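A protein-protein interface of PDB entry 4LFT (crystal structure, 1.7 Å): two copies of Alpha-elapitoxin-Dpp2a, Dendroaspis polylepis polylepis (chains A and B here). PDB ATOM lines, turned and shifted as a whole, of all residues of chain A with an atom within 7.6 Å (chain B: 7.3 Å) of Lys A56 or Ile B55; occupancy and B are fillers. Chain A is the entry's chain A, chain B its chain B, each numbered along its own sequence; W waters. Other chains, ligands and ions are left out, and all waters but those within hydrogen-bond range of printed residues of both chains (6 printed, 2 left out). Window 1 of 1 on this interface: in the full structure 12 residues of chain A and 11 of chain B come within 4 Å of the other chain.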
ATOM      1  N   ILE A  20      -5.143  15.697  15.331  1.00  0.00           N
ATOM      2  CA  ILE A  20      -6.547  15.523  15.633  1.00  0.00           C
ATOM      3  C   ILE A  20      -7.135  16.962  15.531  1.00  0.00           C
ATOM      4  O   ILE A  20      -6.551  17.910  16.021  1.00  0.00           O
ATOM      5  CB  ILE A  20      -6.751  15.023  17.109  1.00  0.00           C
ATOM      6  CG1 ILE A  20      -6.086  13.681  17.326  1.00  0.00           C
ATOM      7  CG2 ILE A  20      -8.213  14.998  17.518  1.00  0.00           C
ATOM      8  CD1 ILE A  20      -6.812  12.611  16.642  1.00  0.00           C
ATOM      9  N   CYS A  21      -8.291  17.063  14.919  1.00  0.00           N
ATOM     10  CA  CYS A  21      -9.138  18.261  15.012  1.00  0.00           C
ATOM     11  C   CYS A  21     -10.221  18.052  16.048  1.00  0.00           C
ATOM     12  O   CYS A  21     -10.728  16.970  16.256  1.00  0.00           O
ATOM     13  CB  CYS A  21      -9.831  18.554  13.664  1.00  0.00           C
ATOM     14  SG  CYS A  21      -8.654  18.707  12.277  1.00  0.00           S
ATOM     15  N   TYR A  22     -10.641  19.156  16.671  1.00  0.00           N
ATOM     16  CA  TYR A  22     -11.637  19.117  17.662  1.00  0.00           C
ATOM     17  C   TYR A  22     -12.581  20.266  17.611  1.00  0.00           C
ATOM     18  O   TYR A  22     -12.271  21.355  17.112  1.00  0.00           O
ATOM     19  CB  TYR A  22     -11.071  18.940  19.097  1.00  0.00           C
ATOM     20  CG  TYR A  22     -10.496  20.165  19.639  1.00  0.00           C
ATOM     21  CD1 TYR A  22     -11.278  21.117  20.320  1.00  0.00           C
ATOM     22  CD2 TYR A  22      -9.152  20.450  19.488  1.00  0.00           C
ATOM     23  CE1 TYR A  22     -10.715  22.313  20.753  1.00  0.00           C
ATOM     24  CE2 TYR A  22      -8.587  21.583  19.966  1.00  0.00           C
ATOM     25  CZ  TYR A  22      -9.375  22.552  20.609  1.00  0.00           C
ATOM     26  OH  TYR A  22      -8.819  23.747  21.016  1.00  0.00           O
ATOM     27  N   THR A  23     -13.760  19.970  18.167  1.00  0.00           N
ATOM     28  CA  THR A  23     -14.799  20.996  18.385  1.00  0.00           C
ATOM     29  C   THR A  23     -15.258  20.853  19.843  1.00  0.00           C
ATOM     30  O   THR A  23     -15.835  19.804  20.195  1.00  0.00           O
ATOM     31  CB  THR A  23     -16.037  20.723  17.519  1.00  0.00           C
ATOM     32  OG1 THR A  23     -15.664  20.680  16.115  1.00  0.00           O
ATOM     33  CG2 THR A  23     -17.126  21.820  17.717  1.00  0.00           C
ATOM     34  N   LYS A  24     -15.063  21.873  20.656  1.00  0.00           N
ATOM     35  CA  LYS A  24     -15.414  21.806  22.069  1.00  0.00           C
ATOM     36  C   LYS A  24     -16.606  22.740  22.200  1.00  0.00           C
ATOM     37  O   LYS A  24     -16.537  23.894  21.668  1.00  0.00           O
ATOM     38  CB  LYS A  24     -14.215  22.263  22.846  1.00  0.00           C
ATOM     39  CG  LYS A  24     -14.350  22.222  24.322  1.00  0.00           C
ATOM     40  CD  LYS A  24     -13.118  22.838  25.035  1.00  0.00           C
ATOM     41  CE  LYS A  24     -11.831  22.083  24.832  1.00  0.00           C
ATOM     42  NZ  LYS A  24     -10.743  22.704  25.701  1.00  0.00           N
ATOM     43  N   THR A  25     -17.713  22.269  22.829  1.00  0.00           N
ATOM     44  CA  THR A  25     -18.912  23.105  23.082  1.00  0.00           C
ATOM     45  C   THR A  25     -19.318  23.040  24.556  1.00  0.00           C
ATOM     46  O   THR A  25     -19.091  22.070  25.251  1.00  0.00           O
ATOM     47  CB  THR A  25     -20.137  22.754  22.197  1.00  0.00           C
ATOM     48  OG1 THR A  25     -20.352  21.335  22.310  1.00  0.00           O
ATOM     49  CG2 THR A  25     -19.838  23.135  20.714  1.00  0.00           C
ATOM     50  N   GLU A  39     -15.160  26.232  20.692  1.00  0.00           N
ATOM     51  CA  GLU A  39     -13.753  26.385  20.395  1.00  0.00           C
ATOM     52  C   GLU A  39     -13.390  25.281  19.416  1.00  0.00           C
ATOM     53  O   GLU A  39     -13.795  24.088  19.606  1.00  0.00           O
ATOM     54  CB  GLU A  39     -12.935  26.186  21.680  1.00  0.00           C
ATOM     55  CG  GLU A  39     -11.452  26.336  21.511  1.00  0.00           C
ATOM     56  CD  GLU A  39     -10.764  25.988  22.830  1.00  0.00           C
ATOM     57  OE1 GLU A  39     -10.948  26.802  23.762  1.00  0.00           O
ATOM     58  OE2 GLU A  39     -10.057  24.943  22.943  1.00  0.00           O
ATOM     59  N   LEU A  40     -12.666  25.672  18.369  1.00  0.00           N
ATOM     60  CA  LEU A  40     -12.205  24.716  17.344  1.00  0.00           C
ATOM     61  C   LEU A  40     -10.680  24.804  17.236  1.00  0.00           C
ATOM     62  O   LEU A  40     -10.127  25.919  17.223  1.00  0.00           O
ATOM     63  CB  LEU A  40     -12.792  25.086  15.997  1.00  0.00           C
ATOM     64  CG  LEU A  40     -14.314  25.284  15.836  1.00  0.00           C
ATOM     65  CD1 LEU A  40     -14.620  26.164  14.645  1.00  0.00           C
ATOM     66  CD2 LEU A  40     -15.010  23.951  15.691  1.00  0.00           C
ATOM     67  N   GLY A  41     -10.048  23.645  17.119  1.00  0.00           N
ATOM     68  CA  GLY A  41      -8.615  23.585  16.948  1.00  0.00           C
ATOM     69  C   GLY A  41      -8.068  22.226  16.582  1.00  0.00           C
ATOM     70  O   GLY A  41      -8.790  21.282  16.224  1.00  0.00           O
ATOM     71  N   CYS A  46      -7.328  13.673  21.569  1.00  0.00           N
ATOM     72  CA  CYS A  46      -8.657  14.282  21.695  1.00  0.00           C
ATOM     73  C   CYS A  46      -8.722  14.864  23.079  1.00  0.00           C
ATOM     74  O   CYS A  46      -8.479  14.103  24.045  1.00  0.00           O
ATOM     75  CB  CYS A  46      -9.725  13.258  21.591  1.00  0.00           C
ATOM     76  SG  CYS A  46     -11.403  13.895  21.693  1.00  0.00           S
ATOM     77  N   PRO A  47      -9.050  16.157  23.215  1.00  0.00           N
ATOM     78  CA  PRO A  47      -9.016  16.760  24.579  1.00  0.00           C
ATOM     79  C   PRO A  47      -9.935  16.126  25.616  1.00  0.00           C
ATOM     80  O   PRO A  47     -11.042  15.751  25.371  1.00  0.00           O
ATOM     81  CB  PRO A  47      -9.462  18.188  24.296  1.00  0.00           C
ATOM     82  CG  PRO A  47      -8.891  18.445  22.892  1.00  0.00           C
ATOM     83  CD  PRO A  47      -9.285  17.199  22.196  1.00  0.00           C
ATOM     84  N   VAL A  49     -12.172  16.849  28.604  1.00  0.00           N
ATOM     85  CA  VAL A  49     -12.921  18.031  29.019  1.00  0.00           C
ATOM     86  C   VAL A  49     -13.718  17.704  30.302  1.00  0.00           C
ATOM     87  O   VAL A  49     -14.212  16.564  30.482  1.00  0.00           O
ATOM     88  CB  VAL A  49     -13.892  18.480  27.900  1.00  0.00           C
ATOM     89  CG1 VAL A  49     -13.060  18.730  26.617  1.00  0.00           C
ATOM     90  CG2 VAL A  49     -15.000  17.445  27.677  1.00  0.00           C
ATOM     91  N   GLU A  54     -18.766  19.328  25.941  1.00  0.00           N
ATOM     92  CA  GLU A  54     -18.891  18.238  24.952  1.00  0.00           C
ATOM     93  C   GLU A  54     -17.720  18.406  23.978  1.00  0.00           C
ATOM     94  O   GLU A  54     -17.251  19.561  23.687  1.00  0.00           O
ATOM     95  CB  GLU A  54     -20.214  18.258  24.240  1.00  0.00           C
ATOM     96  CG  GLU A  54     -21.368  18.220  25.257  1.00  0.00           C
ATOM     97  CD  GLU A  54     -22.696  17.930  24.685  1.00  0.00           C
ATOM     98  OE1 GLU A  54     -22.801  18.029  23.405  1.00  0.00           O
ATOM     99  OE2 GLU A  54     -23.629  17.630  25.565  1.00  0.00           O
ATOM    100  N   ILE A  55     -17.158  17.278  23.547  1.00  0.00           N
ATOM    101  CA  ILE A  55     -15.946  17.346  22.748  1.00  0.00           C
ATOM    102  C   ILE A  55     -16.117  16.399  21.552  1.00  0.00           C
ATOM    103  O   ILE A  55     -16.520  15.222  21.745  1.00  0.00           O
ATOM    104  CB  ILE A  55     -14.689  17.015  23.568  1.00  0.00           C
ATOM    105  CG1 ILE A  55     -13.366  17.140  22.761  1.00  0.00           C
ATOM    106  CG2 ILE A  55     -14.630  15.619  24.128  1.00  0.00           C
ATOM    107  CD1 ILE A  55     -12.884  18.550  22.656  1.00  0.00           C
ATOM    108  N   LYS A  56     -15.887  16.913  20.348  1.00  0.00           N
ATOM    109  CA  LYS A  56     -15.922  16.101  19.130  1.00  0.00           C
ATOM    110  C   LYS A  56     -14.553  16.109  18.436  1.00  0.00           C
ATOM    111  O   LYS A  56     -13.958  17.163  18.203  1.00  0.00           O
ATOM    112  CB  LYS A  56     -17.055  16.438  18.166  1.00  0.00           C
ATOM    113  CG  LYS A  56     -17.070  15.658  16.860  1.00  0.00           C
ATOM    114  CD  LYS A  56     -18.420  15.701  16.141  1.00  0.00           C
ATOM    115  CE  LYS A  56     -18.532  14.789  14.895  1.00  0.00           C
ATOM    116  NZ  LYS A  56     -19.892  14.995  14.209  1.00  0.00           N
ATOM    117  N   CYS A  57     -13.997  14.880  18.219  1.00  0.00           N
ATOM    118  CA  CYS A  57     -12.640  14.697  17.695  1.00  0.00           C
ATOM    119  C   CYS A  57     -12.686  13.843  16.413  1.00  0.00           C
ATOM    120  O   CYS A  57     -13.530  12.888  16.192  1.00  0.00           O
ATOM    121  CB  CYS A  57     -11.760  13.993  18.716  1.00  0.00           C
ATOM    122  SG  CYS A  57     -11.440  15.152  20.061  1.00  0.00           S
ATOM    123  N   CYS A  58     -11.814  14.271  15.520  1.00  0.00           N
ATOM    124  CA  CYS A  58     -11.689  13.620  14.190  1.00  0.00           C
ATOM    125  C   CYS A  58     -10.252  13.832  13.731  1.00  0.00           C
ATOM    126  O   CYS A  58      -9.572  14.687  14.206  1.00  0.00           O
ATOM    127  CB  CYS A  58     -12.751  14.091  13.220  1.00  0.00           C
ATOM    128  SG  CYS A  58     -12.757  15.889  13.034  1.00  0.00           S
ATOM    129  N   SER A  59      -9.781  13.040  12.735  1.00  0.00           N
ATOM    130  CA  SER A  59      -8.380  13.140  12.312  1.00  0.00           C
ATOM    131  C   SER A  59      -8.204  13.104  10.816  1.00  0.00           C
ATOM    132  O   SER A  59      -7.285  12.489  10.300  1.00  0.00           O
ATOM    133  CB  SER A  59      -7.573  12.043  13.002  1.00  0.00           C
ATOM    134  OG  SER A  59      -8.123  10.769  12.696  1.00  0.00           O
ATOM    135  N   CYS A  63     -11.927  18.332   9.351  1.00  0.00           N
ATOM    136  CA  CYS A  63     -13.054  17.516   9.629  1.00  0.00           C
ATOM    137  C   CYS A  63     -13.959  18.089  10.724  1.00  0.00           C
ATOM    138  O   CYS A  63     -15.083  17.612  10.893  1.00  0.00           O
ATOM    139  CB  CYS A  63     -12.608  16.111  10.061  1.00  0.00           C
ATOM    140  SG  CYS A  63     -11.462  16.094  11.454  1.00  0.00           S
ATOM    141  N   ASN A  64     -13.480  19.098  11.428  1.00  0.00           N
ATOM    142  CA  ASN A  64     -14.268  19.770  12.485  1.00  0.00           C
ATOM    143  C   ASN A  64     -15.140  20.865  11.827  1.00  0.00           C
ATOM    144  O   ASN A  64     -14.779  22.010  12.001  1.00  0.00           O
ATOM    145  CB  ASN A  64     -13.347  20.208  13.633  1.00  0.00           C
ATOM    146  CG  ASN A  64     -12.221  21.136  13.216  1.00  0.00           C
ATOM    147  OD1 ASN A  64     -11.837  21.217  12.048  1.00  0.00           O
ATOM    148  ND2 ASN A  64     -11.701  21.900  14.209  1.00  0.00           N
ATOM    149  N   CYS B  21     -20.951   9.482  27.734  1.00  0.00           N
ATOM    150  CA  CYS B  21     -21.774   9.037  26.648  1.00  0.00           C
ATOM    151  C   CYS B  21     -21.094   9.478  25.326  1.00  0.00           C
ATOM    152  O   CYS B  21     -20.344  10.451  25.291  1.00  0.00           O
ATOM    153  CB  CYS B  21     -23.096   9.722  26.624  1.00  0.00           C
ATOM    154  SG  CYS B  21     -24.180   9.446  28.079  1.00  0.00           S
ATOM    155  N   TYR B  22     -21.252   8.613  24.328  1.00  0.00           N
ATOM    156  CA  TYR B  22     -20.535   8.876  23.045  1.00  0.00           C
ATOM    157  C   TYR B  22     -21.415   8.610  21.868  1.00  0.00           C
ATOM    158  O   TYR B  22     -22.396   7.820  21.891  1.00  0.00           O
ATOM    159  CB  TYR B  22     -19.221   8.086  22.940  1.00  0.00           C
ATOM    160  CG  TYR B  22     -19.470   6.625  22.660  1.00  0.00           C
ATOM    161  CD1 TYR B  22     -19.621   6.135  21.338  1.00  0.00           C
ATOM    162  CD2 TYR B  22     -19.423   5.713  23.665  1.00  0.00           C
ATOM    163  CE1 TYR B  22     -19.791   4.782  21.069  1.00  0.00           C
ATOM    164  CE2 TYR B  22     -19.625   4.401  23.458  1.00  0.00           C
ATOM    165  CZ  TYR B  22     -19.784   3.906  22.164  1.00  0.00           C
ATOM    166  OH  TYR B  22     -19.950   2.580  21.940  1.00  0.00           O
ATOM    167  N   THR B  23     -21.084   9.407  20.842  1.00  0.00           N
ATOM    168  CA  THR B  23     -21.615   9.227  19.477  1.00  0.00           C
ATOM    169  C   THR B  23     -20.450   8.987  18.527  1.00  0.00           C
ATOM    170  O   THR B  23     -19.507   9.769  18.361  1.00  0.00           O
ATOM    171  CB  THR B  23     -22.412  10.491  18.989  1.00  0.00           C
ATOM    172  OG1 THR B  23     -23.464  10.859  19.906  1.00  0.00           O
ATOM    173  CG2 THR B  23     -22.980  10.202  17.653  1.00  0.00           C
ATOM    174  N   LYS B  24     -20.425   7.783  17.919  1.00  0.00           N
ATOM    175  CA  LYS B  24     -19.306   7.461  17.047  1.00  0.00           C
ATOM    176  C   LYS B  24     -19.927   7.390  15.618  1.00  0.00           C
ATOM    177  O   LYS B  24     -20.950   6.747  15.445  1.00  0.00           O
ATOM    178  CB  LYS B  24     -18.753   6.059  17.429  1.00  0.00           C
ATOM    179  CG  LYS B  24     -17.670   5.586  16.533  1.00  0.00           C
ATOM    180  CD  LYS B  24     -17.315   4.111  16.739  1.00  0.00           C
ATOM    181  CE  LYS B  24     -16.768   3.793  18.094  1.00  0.00           C
ATOM    182  NZ  LYS B  24     -16.035   2.434  17.931  1.00  0.00           N
ATOM    183  N   THR B  25     -19.331   8.132  14.674  1.00  0.00           N
ATOM    184  CA  THR B  25     -19.855   8.211  13.307  1.00  0.00           C
ATOM    185  C   THR B  25     -18.757   7.978  12.306  1.00  0.00           C
ATOM    186  O   THR B  25     -17.601   8.188  12.530  1.00  0.00           O
ATOM    187  CB  THR B  25     -20.553   9.594  13.055  1.00  0.00           C
ATOM    188  OG1 THR B  25     -19.613  10.581  13.409  1.00  0.00           O
ATOM    189  CG2 THR B  25     -21.823   9.713  13.844  1.00  0.00           C
ATOM    190  N   LYS B  36     -24.295   9.289   7.632  1.00  0.00           N
ATOM    191  CA  LYS B  36     -23.280   8.516   8.407  1.00  0.00           C
ATOM    192  C   LYS B  36     -23.890   7.351   9.118  1.00  0.00           C
ATOM    193  O   LYS B  36     -25.052   7.354   9.501  1.00  0.00           O
ATOM    194  CB  LYS B  36     -22.599   9.408   9.387  1.00  0.00           C
ATOM    195  CG  LYS B  36     -21.702  10.379   8.730  1.00  0.00           C
ATOM    196  CD  LYS B  36     -21.407  11.488   9.627  1.00  0.00           C
ATOM    197  CE  LYS B  36     -20.641  12.536   8.865  1.00  0.00           C
ATOM    198  NZ  LYS B  36     -20.513  13.729   9.768  1.00  0.00           N
ATOM    199  N   GLU B  39     -22.913   4.730  16.004  1.00  0.00           N
ATOM    200  CA  GLU B  39     -23.022   3.961  17.219  1.00  0.00           C
ATOM    201  C   GLU B  39     -23.103   4.897  18.435  1.00  0.00           C
ATOM    202  O   GLU B  39     -22.340   5.902  18.488  1.00  0.00           O
ATOM    203  CB  GLU B  39     -21.726   3.141  17.382  1.00  0.00           C
ATOM    204  CG  GLU B  39     -21.618   2.239  18.604  1.00  0.00           C
ATOM    205  CD  GLU B  39     -20.304   1.450  18.615  1.00  0.00           C
ATOM    206  OE1 GLU B  39     -20.158   0.583  17.732  1.00  0.00           O
ATOM    207  OE2 GLU B  39     -19.435   1.738  19.462  1.00  0.00           O
ATOM    208  N   THR B  45     -13.894   6.355  29.338  1.00  0.00           N
ATOM    209  CA  THR B  45     -13.175   7.448  28.714  1.00  0.00           C
ATOM    210  C   THR B  45     -13.668   7.537  27.256  1.00  0.00           C
ATOM    211  O   THR B  45     -14.183   6.577  26.697  1.00  0.00           O
ATOM    212  CB  THR B  45     -11.646   7.164  28.648  1.00  0.00           C
ATOM    213  OG1 THR B  45     -11.411   5.866  28.073  1.00  0.00           O
ATOM    214  CG2 THR B  45     -11.078   7.167  30.049  1.00  0.00           C
ATOM    215  N   CYS B  46     -13.450   8.676  26.682  1.00  0.00           N
ATOM    216  CA  CYS B  46     -13.910   8.931  25.320  1.00  0.00           C
ATOM    217  C   CYS B  46     -13.166   7.984  24.386  1.00  0.00           C
ATOM    218  O   CYS B  46     -11.938   8.040  24.361  1.00  0.00           O
ATOM    219  CB  CYS B  46     -13.659  10.382  24.979  1.00  0.00           C
ATOM    220  SG  CYS B  46     -14.362  10.846  23.384  1.00  0.00           S
ATOM    221  N   PRO B  47     -13.908   7.183  23.616  1.00  0.00           N
ATOM    222  CA  PRO B  47     -13.236   6.168  22.724  1.00  0.00           C
ATOM    223  C   PRO B  47     -12.223   6.860  21.765  1.00  0.00           C
ATOM    224  O   PRO B  47     -12.492   7.907  21.203  1.00  0.00           O
ATOM    225  CB  PRO B  47     -14.403   5.532  22.006  1.00  0.00           C
ATOM    226  CG  PRO B  47     -15.599   5.612  22.965  1.00  0.00           C
ATOM    227  CD  PRO B  47     -15.380   6.961  23.621  1.00  0.00           C
ATOM    228  N   LYS B  48     -11.040   6.258  21.566  1.00  0.00           N
ATOM    229  CA  LYS B  48     -10.088   6.699  20.578  1.00  0.00           C
ATOM    230  C   LYS B  48     -10.509   6.024  19.297  1.00  0.00           C
ATOM    231  O   LYS B  48     -10.872   4.841  19.295  1.00  0.00           O
ATOM    232  CB  LYS B  48      -8.652   6.236  20.964  1.00  0.00           C
ATOM    233  CG  LYS B  48      -8.124   6.765  22.289  1.00  0.00           C
ATOM    234  CD  LYS B  48      -8.326   8.259  22.367  1.00  0.00           C
ATOM    235  CE  LYS B  48      -7.316   8.958  23.267  1.00  0.00           C
ATOM    236  NZ  LYS B  48      -7.421  10.425  23.038  1.00  0.00           N
ATOM    237  N   VAL B  49     -10.532   6.778  18.217  1.00  0.00           N
ATOM    238  CA  VAL B  49     -11.012   6.247  16.946  1.00  0.00           C
ATOM    239  C   VAL B  49     -10.004   6.623  15.821  1.00  0.00           C
ATOM    240  O   VAL B  49      -9.272   7.656  15.869  1.00  0.00           O
ATOM    241  CB  VAL B  49     -12.448   6.745  16.612  1.00  0.00           C
ATOM    242  CG1 VAL B  49     -13.441   6.294  17.720  1.00  0.00           C
ATOM    243  CG2 VAL B  49     -12.418   8.281  16.467  1.00  0.00           C
ATOM    244  N   VAL B  53     -13.069   8.108  11.236  1.00  0.00           N
ATOM    245  CA  VAL B  53     -14.151   7.875  12.214  1.00  0.00           C
ATOM    246  C   VAL B  53     -14.085   9.109  13.109  1.00  0.00           C
ATOM    247  O   VAL B  53     -12.962   9.579  13.338  1.00  0.00           O
ATOM    248  CB  VAL B  53     -13.910   6.617  13.067  1.00  0.00           C
ATOM    249  CG1 VAL B  53     -15.110   6.485  13.986  1.00  0.00           C
ATOM    250  CG2 VAL B  53     -13.774   5.394  12.125  1.00  0.00           C
ATOM    251  N   GLU B  54     -15.262   9.535  13.599  1.00  0.00           N
ATOM    252  CA  GLU B  54     -15.384  10.762  14.394  1.00  0.00           C
ATOM    253  C   GLU B  54     -16.035  10.317  15.668  1.00  0.00           C
ATOM    254  O   GLU B  54     -16.940   9.462  15.647  1.00  0.00           O
ATOM    255  CB  GLU B  54     -16.175  11.815  13.598  1.00  0.00           C
ATOM    256  CG  GLU B  54     -15.531  11.947  12.247  1.00  0.00           C
ATOM    257  CD  GLU B  54     -15.905  13.201  11.443  1.00  0.00           C
ATOM    258  OE1 GLU B  54     -16.937  13.809  11.764  1.00  0.00           O
ATOM    259  OE2 GLU B  54     -15.098  13.568  10.492  1.00  0.00           O
ATOM    260  N   ILE B  55     -15.682  11.002  16.747  1.00  0.00           N
ATOM    261  CA  ILE B  55     -16.188  10.678  18.079  1.00  0.00           C
ATOM    262  C   ILE B  55     -16.589  11.944  18.833  1.00  0.00           C
ATOM    263  O   ILE B  55     -15.786  12.848  18.848  1.00  0.00           O
ATOM    264  CB  ILE B  55     -15.122   9.834  18.850  1.00  0.00           C
ATOM    265  CG1 ILE B  55     -15.707   9.183  20.115  1.00  0.00           C
ATOM    266  CG2 ILE B  55     -13.854  10.597  19.127  1.00  0.00           C
ATOM    267  CD1 ILE B  55     -16.699   8.125  19.947  1.00  0.00           C
ATOM    268  N   LYS B  56     -17.799  11.955  19.377  1.00  0.00           N
ATOM    269  CA  LYS B  56     -18.284  13.073  20.250  1.00  0.00           C
ATOM    270  C   LYS B  56     -18.615  12.451  21.636  1.00  0.00           C
ATOM    271  O   LYS B  56     -19.370  11.455  21.727  1.00  0.00           O
ATOM    272  CB  LYS B  56     -19.486  13.737  19.649  1.00  0.00           C
ATOM    273  CG  LYS B  56     -19.880  14.963  20.464  1.00  0.00           C
ATOM    274  CD  LYS B  56     -20.970  15.762  19.826  1.00  0.00           C
ATOM    275  CE  LYS B  56     -21.171  17.082  20.594  1.00  0.00           C
ATOM    276  NZ  LYS B  56     -22.169  17.869  19.788  1.00  0.00           N
ATOM    277  N   CYS B  57     -18.029  13.055  22.643  1.00  0.00           N
ATOM    278  CA  CYS B  57     -18.134  12.585  24.055  1.00  0.00           C
ATOM    279  C   CYS B  57     -18.694  13.673  24.927  1.00  0.00           C
ATOM    280  O   CYS B  57     -18.436  14.841  24.743  1.00  0.00           O
ATOM    281  CB  CYS B  57     -16.770  12.165  24.510  1.00  0.00           C
ATOM    282  SG  CYS B  57     -16.311  10.616  23.669  1.00  0.00           S
HETATM  283  O   HOH W   1     -11.554  11.029  11.439  1.00  0.00           O
HETATM  284  O   HOH W   2     -10.194  10.058  14.306  1.00  0.00           O
HETATM  285  O   HOH W   3     -22.607  20.113  21.908  1.00  0.00           O
HETATM  286  O   HOH W   4     -15.908  15.621   9.072  1.00  0.00           O
HETATM  287  O   HOH W   5     -19.515  13.030  12.229  1.00  0.00           O
HETATM  288  O   HOH W   6      -7.441  10.771  20.347  1.00  0.00           O
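Of the 17 printed residues of chain B, 5 touch a printed residue of chain A.
Hydrophobic or aromatic side chains of chain A within 4 Å of the printed part of chain B: Ile A55.
Among the printed residues, Asp or Glu carboxylates within 4 Å of a Lys or Arg side-chain nitrogen of the other chain: Glu A54 with Lys B56.
The backbone carbonyl oxygen of Ile A55 is in hydrogen-bond range of the backbone NH of Cys B57.
The side-chain carboxylate (OE1) of Glu A54 lies within salt-bridge range of the side-chain amino group (NZ) of Lys B56, at 3.7 Å.
The backbone NH (N) of Cys A57 sits at hydrogen-bond distance from the backbone carbonyl oxygen (O) of Ile B55.
The side-chain sulfur (SG) of Cys A63 forms a disulfide with the side-chain sulfur (SG) of Cys A58 (2.1 Å).
The backbone carbonyl oxygen (O) of Lys B56 is in hydrogen-bond range of the backbone NH (N) of Thr B23, at 2.8 Å.
O of Thr A25 lies within hydrogen-bond range of N of Glu A54, 2.8 Å away.
N of Thr A23 lies within hydrogen-bond range of O of Lys A56 (2.8 Å).
The backbone NH of Cys A21 lies within hydrogen-bond range of the backbone carbonyl oxygen of Cys A58.
The side-chain sulfur (SG) of Cys A57 is disulfide-bonded to the side-chain sulfur (SG) of Cys A46.
Water W3 lies within hydrogen-bond range of the side-chain carboxylate of Glu A54, the side-chain hydroxyl of Thr A25 and the side-chain amino group of Lys B56.
Water W4 bridges the side-chain carboxylate of Glu B54 (2.6 Å) and the backbone carbonyl oxygen of Cys A63 (2.8 Å).
Water W6 lies within hydrogen-bond range of NZ of Lys B48 (2.7 Å) and N of Cys A46 (3.2 Å).
Water W2 lies within hydrogen-bond range of the side-chain hydroxyl of Ser A59 (2.7 Å), the backbone carbonyl oxygen of Val B53 (3.0 Å) and the backbone carbonyl oxygen of Val B49 (3.0 Å).
Water W5 lies within hydrogen-bond range of the side-chain hydroxyl (OG1) of Thr B25 (2.7 Å), the side-chain carboxylate (OE1) of Glu B54 (2.7 Å), the side-chain amino group (NZ) of Lys B36 (2.7 Å) and the side-chain amino group (NZ) of Lys A56 (2.8 Å).
Water W1 bridges the backbone carbonyl oxygen (O) of Val B53 (2.8 Å) and the backbone NH (N) of Ser A59 (3.0 Å).
Glu A54 touches Lys B56, and with the chains exchanged Lys A56 touches Glu B54.
Glu A54 touches Cys B57, and with the chains exchanged Cys A57 touches Glu B54.
Ile B55 touches its own counterpart, Ile A55.
Lys A56 touches its own counterpart, Lys B56.
Positions printed for both chains: 21, 22, 23, 24, 25, 39, 46, 47, 49, 54, 55, 56 and 57.
Of the 13 pairs that touch across the chains among the printed residues, 10 have their exchanged pair printed and touching as well.
NZ of Lys B48 touches N of Cys A46, at 3.6 Å.
Glu A54 touches Cys B57 (CA to O, 3.4 Å).
O of Ile B55 touches O of Ile A55, at 3.8 Å.
Ile A55 touches Lys B56 (O to CA, 3.2 Å).
Lys A56 touches Glu B54.
O of Ile B55 touches CA of Lys A56 (3.3 Å).
Lys B56 touches Lys A56 (CB to CB, 3.9 Å).
O of Cys A57 touches CA of Glu B54, 3.3 Å away.
OE2 of Glu B54 touches CB of Cys A58, 3.6 Å away.
OE2 of Glu B54 touches CB of Cys A63 (3.6 Å).
Of chain B, only Glu B54 (3.6 Å), Ile B55 (3.3 Å) and Lys B56 (3.9 Å) come within 4 Å of Lys A56.
Printed residues of chain B within 4 Å of Cys A58: Glu B54.
Thr B45 touches none of the printed residues of chain A.
Ile B55 touches just these residues of chain A: Ile A55, Lys A56 and Cys A57.
Of the printed residues of chain A, Lys B56 touches Glu A54, Ile A55 and Lys A56.
The nearest residue of chain B that does not touch Lys A56 is Thr B25 (4.5 Å).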
